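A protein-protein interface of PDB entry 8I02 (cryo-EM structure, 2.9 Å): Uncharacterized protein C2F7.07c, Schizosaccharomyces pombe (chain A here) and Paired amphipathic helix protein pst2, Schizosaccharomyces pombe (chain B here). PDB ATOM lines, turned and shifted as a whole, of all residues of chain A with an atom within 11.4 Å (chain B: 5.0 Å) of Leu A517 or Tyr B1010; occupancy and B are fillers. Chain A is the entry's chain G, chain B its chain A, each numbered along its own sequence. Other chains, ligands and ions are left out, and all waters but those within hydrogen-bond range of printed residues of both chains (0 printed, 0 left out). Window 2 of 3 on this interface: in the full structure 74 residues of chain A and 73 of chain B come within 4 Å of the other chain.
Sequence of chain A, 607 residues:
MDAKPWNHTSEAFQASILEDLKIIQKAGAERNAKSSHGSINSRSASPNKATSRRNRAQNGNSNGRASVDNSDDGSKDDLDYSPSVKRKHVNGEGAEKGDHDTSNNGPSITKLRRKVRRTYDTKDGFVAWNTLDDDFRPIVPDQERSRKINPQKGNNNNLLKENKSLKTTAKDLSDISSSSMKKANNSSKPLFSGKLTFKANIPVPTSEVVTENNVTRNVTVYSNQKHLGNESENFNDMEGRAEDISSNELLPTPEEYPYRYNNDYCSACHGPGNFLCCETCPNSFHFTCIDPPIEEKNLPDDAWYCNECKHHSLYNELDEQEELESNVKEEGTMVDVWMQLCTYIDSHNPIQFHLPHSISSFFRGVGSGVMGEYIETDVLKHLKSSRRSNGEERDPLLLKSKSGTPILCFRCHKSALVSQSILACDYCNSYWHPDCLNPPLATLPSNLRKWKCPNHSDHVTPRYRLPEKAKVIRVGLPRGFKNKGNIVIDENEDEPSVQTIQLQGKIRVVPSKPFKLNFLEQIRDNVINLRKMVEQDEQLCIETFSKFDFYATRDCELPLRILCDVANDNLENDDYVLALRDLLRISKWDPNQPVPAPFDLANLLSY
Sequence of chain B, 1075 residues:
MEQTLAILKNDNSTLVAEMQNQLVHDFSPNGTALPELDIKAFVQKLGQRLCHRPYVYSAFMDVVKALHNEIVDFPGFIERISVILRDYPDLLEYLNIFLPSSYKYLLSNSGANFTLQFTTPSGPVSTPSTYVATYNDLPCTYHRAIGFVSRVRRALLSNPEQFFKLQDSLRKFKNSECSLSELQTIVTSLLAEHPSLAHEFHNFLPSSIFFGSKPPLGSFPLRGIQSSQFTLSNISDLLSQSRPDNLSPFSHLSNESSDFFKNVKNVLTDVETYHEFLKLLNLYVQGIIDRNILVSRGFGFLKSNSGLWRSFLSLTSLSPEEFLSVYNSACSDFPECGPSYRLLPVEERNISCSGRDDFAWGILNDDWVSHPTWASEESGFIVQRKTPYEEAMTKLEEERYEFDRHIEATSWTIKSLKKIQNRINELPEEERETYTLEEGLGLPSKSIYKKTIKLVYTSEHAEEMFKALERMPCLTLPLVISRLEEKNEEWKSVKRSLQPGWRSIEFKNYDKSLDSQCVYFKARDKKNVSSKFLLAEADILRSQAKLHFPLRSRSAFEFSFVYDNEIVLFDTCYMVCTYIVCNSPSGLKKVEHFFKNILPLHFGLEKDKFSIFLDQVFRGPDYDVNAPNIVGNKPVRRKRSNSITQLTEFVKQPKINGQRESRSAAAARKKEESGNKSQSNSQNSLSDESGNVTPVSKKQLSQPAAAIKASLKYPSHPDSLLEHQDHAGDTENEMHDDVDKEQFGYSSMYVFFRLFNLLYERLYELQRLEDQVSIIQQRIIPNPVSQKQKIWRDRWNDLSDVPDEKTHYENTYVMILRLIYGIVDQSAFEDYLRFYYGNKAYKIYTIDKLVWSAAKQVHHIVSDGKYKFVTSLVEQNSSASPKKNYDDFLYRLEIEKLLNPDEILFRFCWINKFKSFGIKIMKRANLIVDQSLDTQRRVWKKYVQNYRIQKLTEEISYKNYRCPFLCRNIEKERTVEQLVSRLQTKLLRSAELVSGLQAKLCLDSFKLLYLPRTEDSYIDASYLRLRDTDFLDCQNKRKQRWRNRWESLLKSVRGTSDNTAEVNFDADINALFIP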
ATOM      1  N   PHE A 515     -25.383 -21.040  -4.023  1.00  0.00           N
ATOM      2  CA  PHE A 515     -26.039 -20.072  -4.892  1.00  0.00           C
ATOM      3  C   PHE A 515     -24.979 -19.178  -5.509  1.00  0.00           C
ATOM      4  O   PHE A 515     -24.242 -18.497  -4.797  1.00  0.00           O
ATOM      5  CB  PHE A 515     -27.065 -19.256  -4.114  1.00  0.00           C
ATOM      6  CG  PHE A 515     -27.903 -20.079  -3.190  1.00  0.00           C
ATOM      7  CD1 PHE A 515     -28.231 -19.606  -1.936  1.00  0.00           C
ATOM      8  CD2 PHE A 515     -28.356 -21.330  -3.570  1.00  0.00           C
ATOM      9  CE1 PHE A 515     -28.996 -20.360  -1.078  1.00  0.00           C
ATOM     10  CE2 PHE A 515     -29.121 -22.090  -2.721  1.00  0.00           C
ATOM     11  CZ  PHE A 515     -29.443 -21.606  -1.471  1.00  0.00           C
ATOM     12  N   LYS A 516     -24.930 -19.206  -6.842  1.00  0.00           N
ATOM     13  CA  LYS A 516     -23.821 -18.761  -7.680  1.00  0.00           C
ATOM     14  C   LYS A 516     -22.679 -19.767  -7.616  1.00  0.00           C
ATOM     15  O   LYS A 516     -21.765 -19.717  -8.442  1.00  0.00           O
ATOM     16  CB  LYS A 516     -23.325 -17.370  -7.279  1.00  0.00           C
ATOM     17  CG  LYS A 516     -23.952 -16.239  -8.050  1.00  0.00           C
ATOM     18  CD  LYS A 516     -23.323 -16.097  -9.420  1.00  0.00           C
ATOM     19  CE  LYS A 516     -21.854 -15.726  -9.310  1.00  0.00           C
ATOM     20  NZ  LYS A 516     -21.657 -14.489  -8.502  1.00  0.00           N
ATOM     21  N   LEU A 517     -22.751 -20.700  -6.661  1.00  0.00           N
ATOM     22  CA  LEU A 517     -21.924 -21.901  -6.586  1.00  0.00           C
ATOM     23  C   LEU A 517     -20.509 -21.702  -7.108  1.00  0.00           C
ATOM     24  O   LEU A 517     -20.041 -22.491  -7.931  1.00  0.00           O
ATOM     25  CB  LEU A 517     -22.607 -23.043  -7.340  1.00  0.00           C
ATOM     26  CG  LEU A 517     -24.029 -23.379  -6.878  1.00  0.00           C
ATOM     27  CD1 LEU A 517     -24.632 -24.441  -7.753  1.00  0.00           C
ATOM     28  CD2 LEU A 517     -24.043 -23.826  -5.439  1.00  0.00           C
ATOM     29  N   ASN A 518     -19.823 -20.656  -6.652  1.00  0.00           N
ATOM     30  CA  ASN A 518     -18.535 -20.239  -7.211  1.00  0.00           C
ATOM     31  C   ASN A 518     -17.446 -20.375  -6.156  1.00  0.00           C
ATOM     32  O   ASN A 518     -17.087 -19.401  -5.493  1.00  0.00           O
ATOM     33  CB  ASN A 518     -18.616 -18.812  -7.712  1.00  0.00           C
ATOM     34  CG  ASN A 518     -19.152 -17.857  -6.670  1.00  0.00           C
ATOM     35  OD1 ASN A 518     -19.914 -18.247  -5.785  1.00  0.00           O
ATOM     36  ND2 ASN A 518     -18.744 -16.597  -6.760  1.00  0.00           N
ATOM     37  N   PHE A 519     -16.887 -21.572  -6.024  1.00  0.00           N
ATOM     38  CA  PHE A 519     -15.854 -21.788  -5.022  1.00  0.00           C
ATOM     39  C   PHE A 519     -14.463 -21.514  -5.570  1.00  0.00           C
ATOM     40  O   PHE A 519     -13.614 -20.962  -4.861  1.00  0.00           O
ATOM     41  CB  PHE A 519     -15.949 -23.210  -4.478  1.00  0.00           C
ATOM     42  CG  PHE A 519     -17.342 -23.616  -4.099  1.00  0.00           C
ATOM     43  CD1 PHE A 519     -17.963 -23.070  -2.998  1.00  0.00           C
ATOM     44  CD2 PHE A 519     -18.031 -24.546  -4.846  1.00  0.00           C
ATOM     45  CE1 PHE A 519     -19.237 -23.445  -2.657  1.00  0.00           C
ATOM     46  CE2 PHE A 519     -19.304 -24.922  -4.511  1.00  0.00           C
ATOM     47  CZ  PHE A 519     -19.909 -24.373  -3.417  1.00  0.00           C
ATOM     48  N   LEU A 520     -14.217 -21.874  -6.829  1.00  0.00           N
ATOM     49  CA  LEU A 520     -12.949 -21.522  -7.457  1.00  0.00           C
ATOM     50  C   LEU A 520     -12.786 -20.012  -7.556  1.00  0.00           C
ATOM     51  O   LEU A 520     -11.696 -19.479  -7.304  1.00  0.00           O
ATOM     52  CB  LEU A 520     -12.855 -22.167  -8.837  1.00  0.00           C
ATOM     53  CG  LEU A 520     -12.080 -23.482  -8.919  1.00  0.00           C
ATOM     54  CD1 LEU A 520     -12.511 -24.432  -7.826  1.00  0.00           C
ATOM     55  CD2 LEU A 520     -12.256 -24.123 -10.281  1.00  0.00           C
ATOM     56  N   GLU A 521     -13.857 -19.301  -7.911  1.00  0.00           N
ATOM     57  CA  GLU A 521     -13.786 -17.848  -7.943  1.00  0.00           C
ATOM     58  C   GLU A 521     -13.513 -17.280  -6.559  1.00  0.00           C
ATOM     59  O   GLU A 521     -12.777 -16.301  -6.423  1.00  0.00           O
ATOM     60  CB  GLU A 521     -15.070 -17.255  -8.517  1.00  0.00           C
ATOM     61  CG  GLU A 521     -15.076 -17.100 -10.035  1.00  0.00           C
ATOM     62  CD  GLU A 521     -13.939 -16.235 -10.566  1.00  0.00           C
ATOM     63  OE1 GLU A 521     -13.514 -16.452 -11.719  1.00  0.00           O
ATOM     64  OE2 GLU A 521     -13.463 -15.341  -9.834  1.00  0.00           O
ATOM     65  N   GLN A 522     -14.076 -17.893  -5.514  1.00  0.00           N
ATOM     66  CA  GLN A 522     -13.827 -17.407  -4.159  1.00  0.00           C
ATOM     67  C   GLN A 522     -12.368 -17.589  -3.753  1.00  0.00           C
ATOM     68  O   GLN A 522     -11.761 -16.685  -3.159  1.00  0.00           O
ATOM     69  CB  GLN A 522     -14.752 -18.113  -3.172  1.00  0.00           C
ATOM     70  CG  GLN A 522     -16.163 -17.570  -3.166  1.00  0.00           C
ATOM     71  CD  GLN A 522     -17.064 -18.297  -2.193  1.00  0.00           C
ATOM     72  OE1 GLN A 522     -16.661 -18.615  -1.077  1.00  0.00           O
ATOM     73  NE2 GLN A 522     -18.294 -18.572  -2.613  1.00  0.00           N
ATOM     74  N   ILE A 523     -11.783 -18.744  -4.064  1.00  0.00           N
ATOM     75  CA  ILE A 523     -10.381 -18.982  -3.733  1.00  0.00           C
ATOM     76  C   ILE A 523      -9.474 -18.011  -4.484  1.00  0.00           C
ATOM     77  O   ILE A 523      -8.530 -17.446  -3.912  1.00  0.00           O
ATOM     78  CB  ILE A 523     -10.022 -20.449  -4.022  1.00  0.00           C
ATOM     79  CG1 ILE A 523     -10.895 -21.368  -3.178  1.00  0.00           C
ATOM     80  CG2 ILE A 523      -8.556 -20.716  -3.756  1.00  0.00           C
ATOM     81  CD1 ILE A 523     -10.703 -22.810  -3.474  1.00  0.00           C
ATOM     82  N   ASP A 525     -10.331 -15.047  -5.618  1.00  0.00           N
ATOM     83  CA  ASP A 525     -10.598 -13.788  -4.938  1.00  0.00           C
ATOM     84  C   ASP A 525      -9.661 -13.603  -3.759  1.00  0.00           C
ATOM     85  O   ASP A 525      -8.956 -12.592  -3.655  1.00  0.00           O
ATOM     86  CB  ASP A 525     -12.052 -13.784  -4.448  1.00  0.00           C
ATOM     87  CG  ASP A 525     -13.048 -13.412  -5.532  1.00  0.00           C
ATOM     88  OD1 ASP A 525     -12.681 -13.439  -6.723  1.00  0.00           O
ATOM     89  OD2 ASP A 525     -14.210 -13.115  -5.189  1.00  0.00           O
ATOM     90  N   SER B 995     -17.332 -18.892 -14.068  1.00  0.00           N
ATOM     91  CA  SER B 995     -18.206 -19.388 -13.014  1.00  0.00           C
ATOM     92  C   SER B 995     -19.599 -18.793 -13.101  1.00  0.00           C
ATOM     93  O   SER B 995     -20.147 -18.319 -12.105  1.00  0.00           O
ATOM     94  CB  SER B 995     -17.618 -19.119 -11.637  1.00  0.00           C
ATOM     95  OG  SER B 995     -18.661 -18.954 -10.700  1.00  0.00           O
ATOM     96  N   LEU B 997     -22.449 -20.290 -13.533  1.00  0.00           N
ATOM     97  CA  LEU B 997     -23.455 -21.177 -12.962  1.00  0.00           C
ATOM     98  C   LEU B 997     -23.947 -20.712 -11.602  1.00  0.00           C
ATOM     99  O   LEU B 997     -23.154 -20.477 -10.686  1.00  0.00           O
ATOM    100  CB  LEU B 997     -22.878 -22.588 -12.850  1.00  0.00           C
ATOM    101  CG  LEU B 997     -23.808 -23.660 -12.284  1.00  0.00           C
ATOM    102  CD1 LEU B 997     -24.530 -24.385 -13.399  1.00  0.00           C
ATOM    103  CD2 LEU B 997     -23.019 -24.635 -11.453  1.00  0.00           C
ATOM    104  N   GLN B 998     -25.267 -20.587 -11.471  1.00  0.00           N
ATOM    105  CA  GLN B 998     -25.937 -20.335 -10.203  1.00  0.00           C
ATOM    106  C   GLN B 998     -27.059 -21.347 -10.030  1.00  0.00           C
ATOM    107  O   GLN B 998     -27.356 -22.136 -10.928  1.00  0.00           O
ATOM    108  CB  GLN B 998     -26.494 -18.908 -10.120  1.00  0.00           C
ATOM    109  CG  GLN B 998     -27.611 -18.620 -11.090  1.00  0.00           C
ATOM    110  CD  GLN B 998     -28.541 -17.531 -10.600  1.00  0.00           C
ATOM    111  OE1 GLN B 998     -28.656 -17.292  -9.398  1.00  0.00           O
ATOM    112  NE2 GLN B 998     -29.219 -16.870 -11.530  1.00  0.00           N
ATOM    113  N   ALA B 999     -27.689 -21.323  -8.864  1.00  0.00           N
ATOM    114  CA  ALA B 999     -28.760 -22.262  -8.563  1.00  0.00           C
ATOM    115  C   ALA B 999     -29.617 -21.680  -7.450  1.00  0.00           C
ATOM    116  O   ALA B 999     -29.510 -20.496  -7.115  1.00  0.00           O
ATOM    117  CB  ALA B 999     -28.196 -23.635  -8.187  1.00  0.00           C
ATOM    118  N   LYS B1000     -30.477 -22.516  -6.877  1.00  0.00           N
ATOM    119  CA  LYS B1000     -31.330 -22.116  -5.769  1.00  0.00           C
ATOM    120  C   LYS B1000     -31.768 -23.373  -5.035  1.00  0.00           C
ATOM    121  O   LYS B1000     -31.731 -24.472  -5.592  1.00  0.00           O
ATOM    122  CB  LYS B1000     -32.539 -21.311  -6.256  1.00  0.00           C
ATOM    123  CG  LYS B1000     -33.337 -20.633  -5.153  1.00  0.00           C
ATOM    124  CD  LYS B1000     -32.479 -19.672  -4.350  1.00  0.00           C
ATOM    125  CE  LYS B1000     -33.282 -19.005  -3.242  1.00  0.00           C
ATOM    126  NZ  LYS B1000     -33.677 -19.958  -2.175  1.00  0.00           N
ATOM    127  N   LEU B1008     -30.851 -28.896  -5.159  1.00  0.00           N
ATOM    128  CA  LEU B1008     -30.456 -27.720  -5.917  1.00  0.00           C
ATOM    129  C   LEU B1008     -31.264 -27.617  -7.205  1.00  0.00           C
ATOM    130  O   LEU B1008     -31.580 -28.624  -7.841  1.00  0.00           O
ATOM    131  CB  LEU B1008     -28.963 -27.766  -6.240  1.00  0.00           C
ATOM    132  CG  LEU B1008     -27.976 -27.800  -5.073  1.00  0.00           C
ATOM    133  CD1 LEU B1008     -26.562 -27.934  -5.597  1.00  0.00           C
ATOM    134  CD2 LEU B1008     -28.104 -26.565  -4.200  1.00  0.00           C
ATOM    135  N   LEU B1009     -31.604 -26.387  -7.580  1.00  0.00           N
ATOM    136  CA  LEU B1009     -32.321 -26.093  -8.819  1.00  0.00           C
ATOM    137  C   LEU B1009     -31.444 -25.151  -9.633  1.00  0.00           C
ATOM    138  O   LEU B1009     -31.421 -23.944  -9.378  1.00  0.00           O
ATOM    139  CB  LEU B1009     -33.683 -25.467  -8.549  1.00  0.00           C
ATOM    140  CG  LEU B1009     -34.716 -26.189  -7.687  1.00  0.00           C
ATOM    141  CD1 LEU B1009     -34.712 -27.689  -7.941  1.00  0.00           C
ATOM    142  CD2 LEU B1009     -34.478 -25.879  -6.227  1.00  0.00           C
ATOM    143  N   TYR B1010     -30.726 -25.695 -10.608  1.00  0.00           N
ATOM    144  CA  TYR B1010     -29.809 -24.892 -11.409  1.00  0.00           C
ATOM    145  C   TYR B1010     -30.604 -24.072 -12.419  1.00  0.00           C
ATOM    146  O   TYR B1010     -31.240 -24.629 -13.317  1.00  0.00           O
ATOM    147  CB  TYR B1010     -28.800 -25.795 -12.107  1.00  0.00           C
ATOM    148  CG  TYR B1010     -27.830 -26.474 -11.168  1.00  0.00           C
ATOM    149  CD1 TYR B1010     -26.512 -26.055 -11.077  1.00  0.00           C
ATOM    150  CD2 TYR B1010     -28.230 -27.537 -10.374  1.00  0.00           C
ATOM    151  CE1 TYR B1010     -25.628 -26.673 -10.228  1.00  0.00           C
ATOM    152  CE2 TYR B1010     -27.352 -28.155  -9.518  1.00  0.00           C
ATOM    153  CZ  TYR B1010     -26.053 -27.717  -9.451  1.00  0.00           C
ATOM    154  OH  TYR B1010     -25.174 -28.334  -8.602  1.00  0.00           O
ATOM    155  N   LEU B1011     -30.568 -22.755 -12.275  1.00  0.00           N
ATOM    156  CA  LEU B1011     -31.319 -21.887 -13.172  1.00  0.00           C
ATOM    157  C   LEU B1011     -30.722 -21.938 -14.575  1.00  0.00           C
ATOM    158  O   LEU B1011     -29.503 -21.801 -14.732  1.00  0.00           O
ATOM    159  CB  LEU B1011     -31.338 -20.457 -12.643  1.00  0.00           C
ATOM    160  CG  LEU B1011     -31.815 -20.277 -11.200  1.00  0.00           C
ATOM    161  CD1 LEU B1011     -32.286 -18.856 -10.979  1.00  0.00           C
ATOM    162  CD2 LEU B1011     -32.928 -21.248 -10.849  1.00  0.00           C
ATOM    163  N   PRO B1012     -31.542 -22.116 -15.612  1.00  0.00           N
ATOM    164  CA  PRO B1012     -31.011 -22.466 -16.936  1.00  0.00           C
ATOM    165  C   PRO B1012     -30.187 -21.347 -17.549  1.00  0.00           C
ATOM    166  O   PRO B1012     -30.178 -20.218 -17.060  1.00  0.00           O
ATOM    167  CB  PRO B1012     -32.274 -22.747 -17.757  1.00  0.00           C
ATOM    168  CG  PRO B1012     -33.339 -23.020 -16.741  1.00  0.00           C
ATOM    169  CD  PRO B1012     -33.012 -22.125 -15.593  1.00  0.00           C
ATOM    170  N   ASP B1016     -20.609 -23.143 -16.059  1.00  0.00           N
ATOM    171  CA  ASP B1016     -19.308 -22.975 -15.426  1.00  0.00           C
ATOM    172  C   ASP B1016     -18.280 -23.738 -16.247  1.00  0.00           C
ATOM    173  O   ASP B1016     -18.591 -24.795 -16.800  1.00  0.00           O
ATOM    174  CB  ASP B1016     -19.328 -23.491 -13.986  1.00  0.00           C
ATOM    175  CG  ASP B1016     -18.096 -23.092 -13.195  1.00  0.00           C
ATOM    176  OD1 ASP B1016     -18.249 -22.368 -12.189  1.00  0.00           O
ATOM    177  OD2 ASP B1016     -16.977 -23.502 -13.568  1.00  0.00           O
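The backbone carbonyl oxygen (O) of Lys A516 lies close to the backbone carbonyl oxygen (O) of Leu B997 (2.7 Å).
O of Lys B1000 sits at hydrogen-bond distance from N of Leu B1009 (2.8 Å). The side-chain amide nitrogen (NE2) of Gln A522 sits close to the backbone carbonyl oxygen (O) of Asn A518, 3.2 Å away.
Among the printed residues, pairs that only touch across the chains: Asn A518 with Ser B995 (3.0 Å), Leu A517 with Tyr B1010 (3.5 Å), Glu A521 with Ser B995 (3.6 Å), Lys A516 with Gln B998 (3.6 Å), Leu A517 with Ala B999 (3.7 Å), Phe A515 with Lys B1000 (3.7 Å), Phe A515 with Ala B999 (3.8 Å) and Lys A516 with Ser B995 (3.9 Å).
Printed residues of chain B within 4 Å of Lys A516: Ser B995 (3.9 Å), Leu B997 (2.7 Å) and Gln B998 (3.6 Å). Leu A517 touches two residues of chain B. Printed residues of chain B within 4 Å of Asn A518: Ser B995. Phe A519 touches none of the printed residues of chain B. Of the printed residues of chain B, Glu A521 touches Ser B995. Leu B997 touches just one residue of chain A: Lys A516. Printed residues of chain A within 4 Å of Gln B998: Lys A516 (3.6 Å). No residue of chain A comes within 4 Å of Leu B1008. No residue of chain A comes within 4 Å of Leu B1009. Of chain A, only Leu A517 comes within 4 Å of Tyr B1010. No residue of chain A comes within 4 Å of Pro B1012. The nearest printed residue of chain A that does not touch Tyr B1010 is Phe A519 (7.9 Å).
Printed residues of chain B that touch a printed residue of chain A: Ser B995, Leu B997, Gln B998, Ala B999, Lys B1000 and Tyr B1010. Of the 10 printed residues of chain A, 5 touch a printed residue of chain B.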
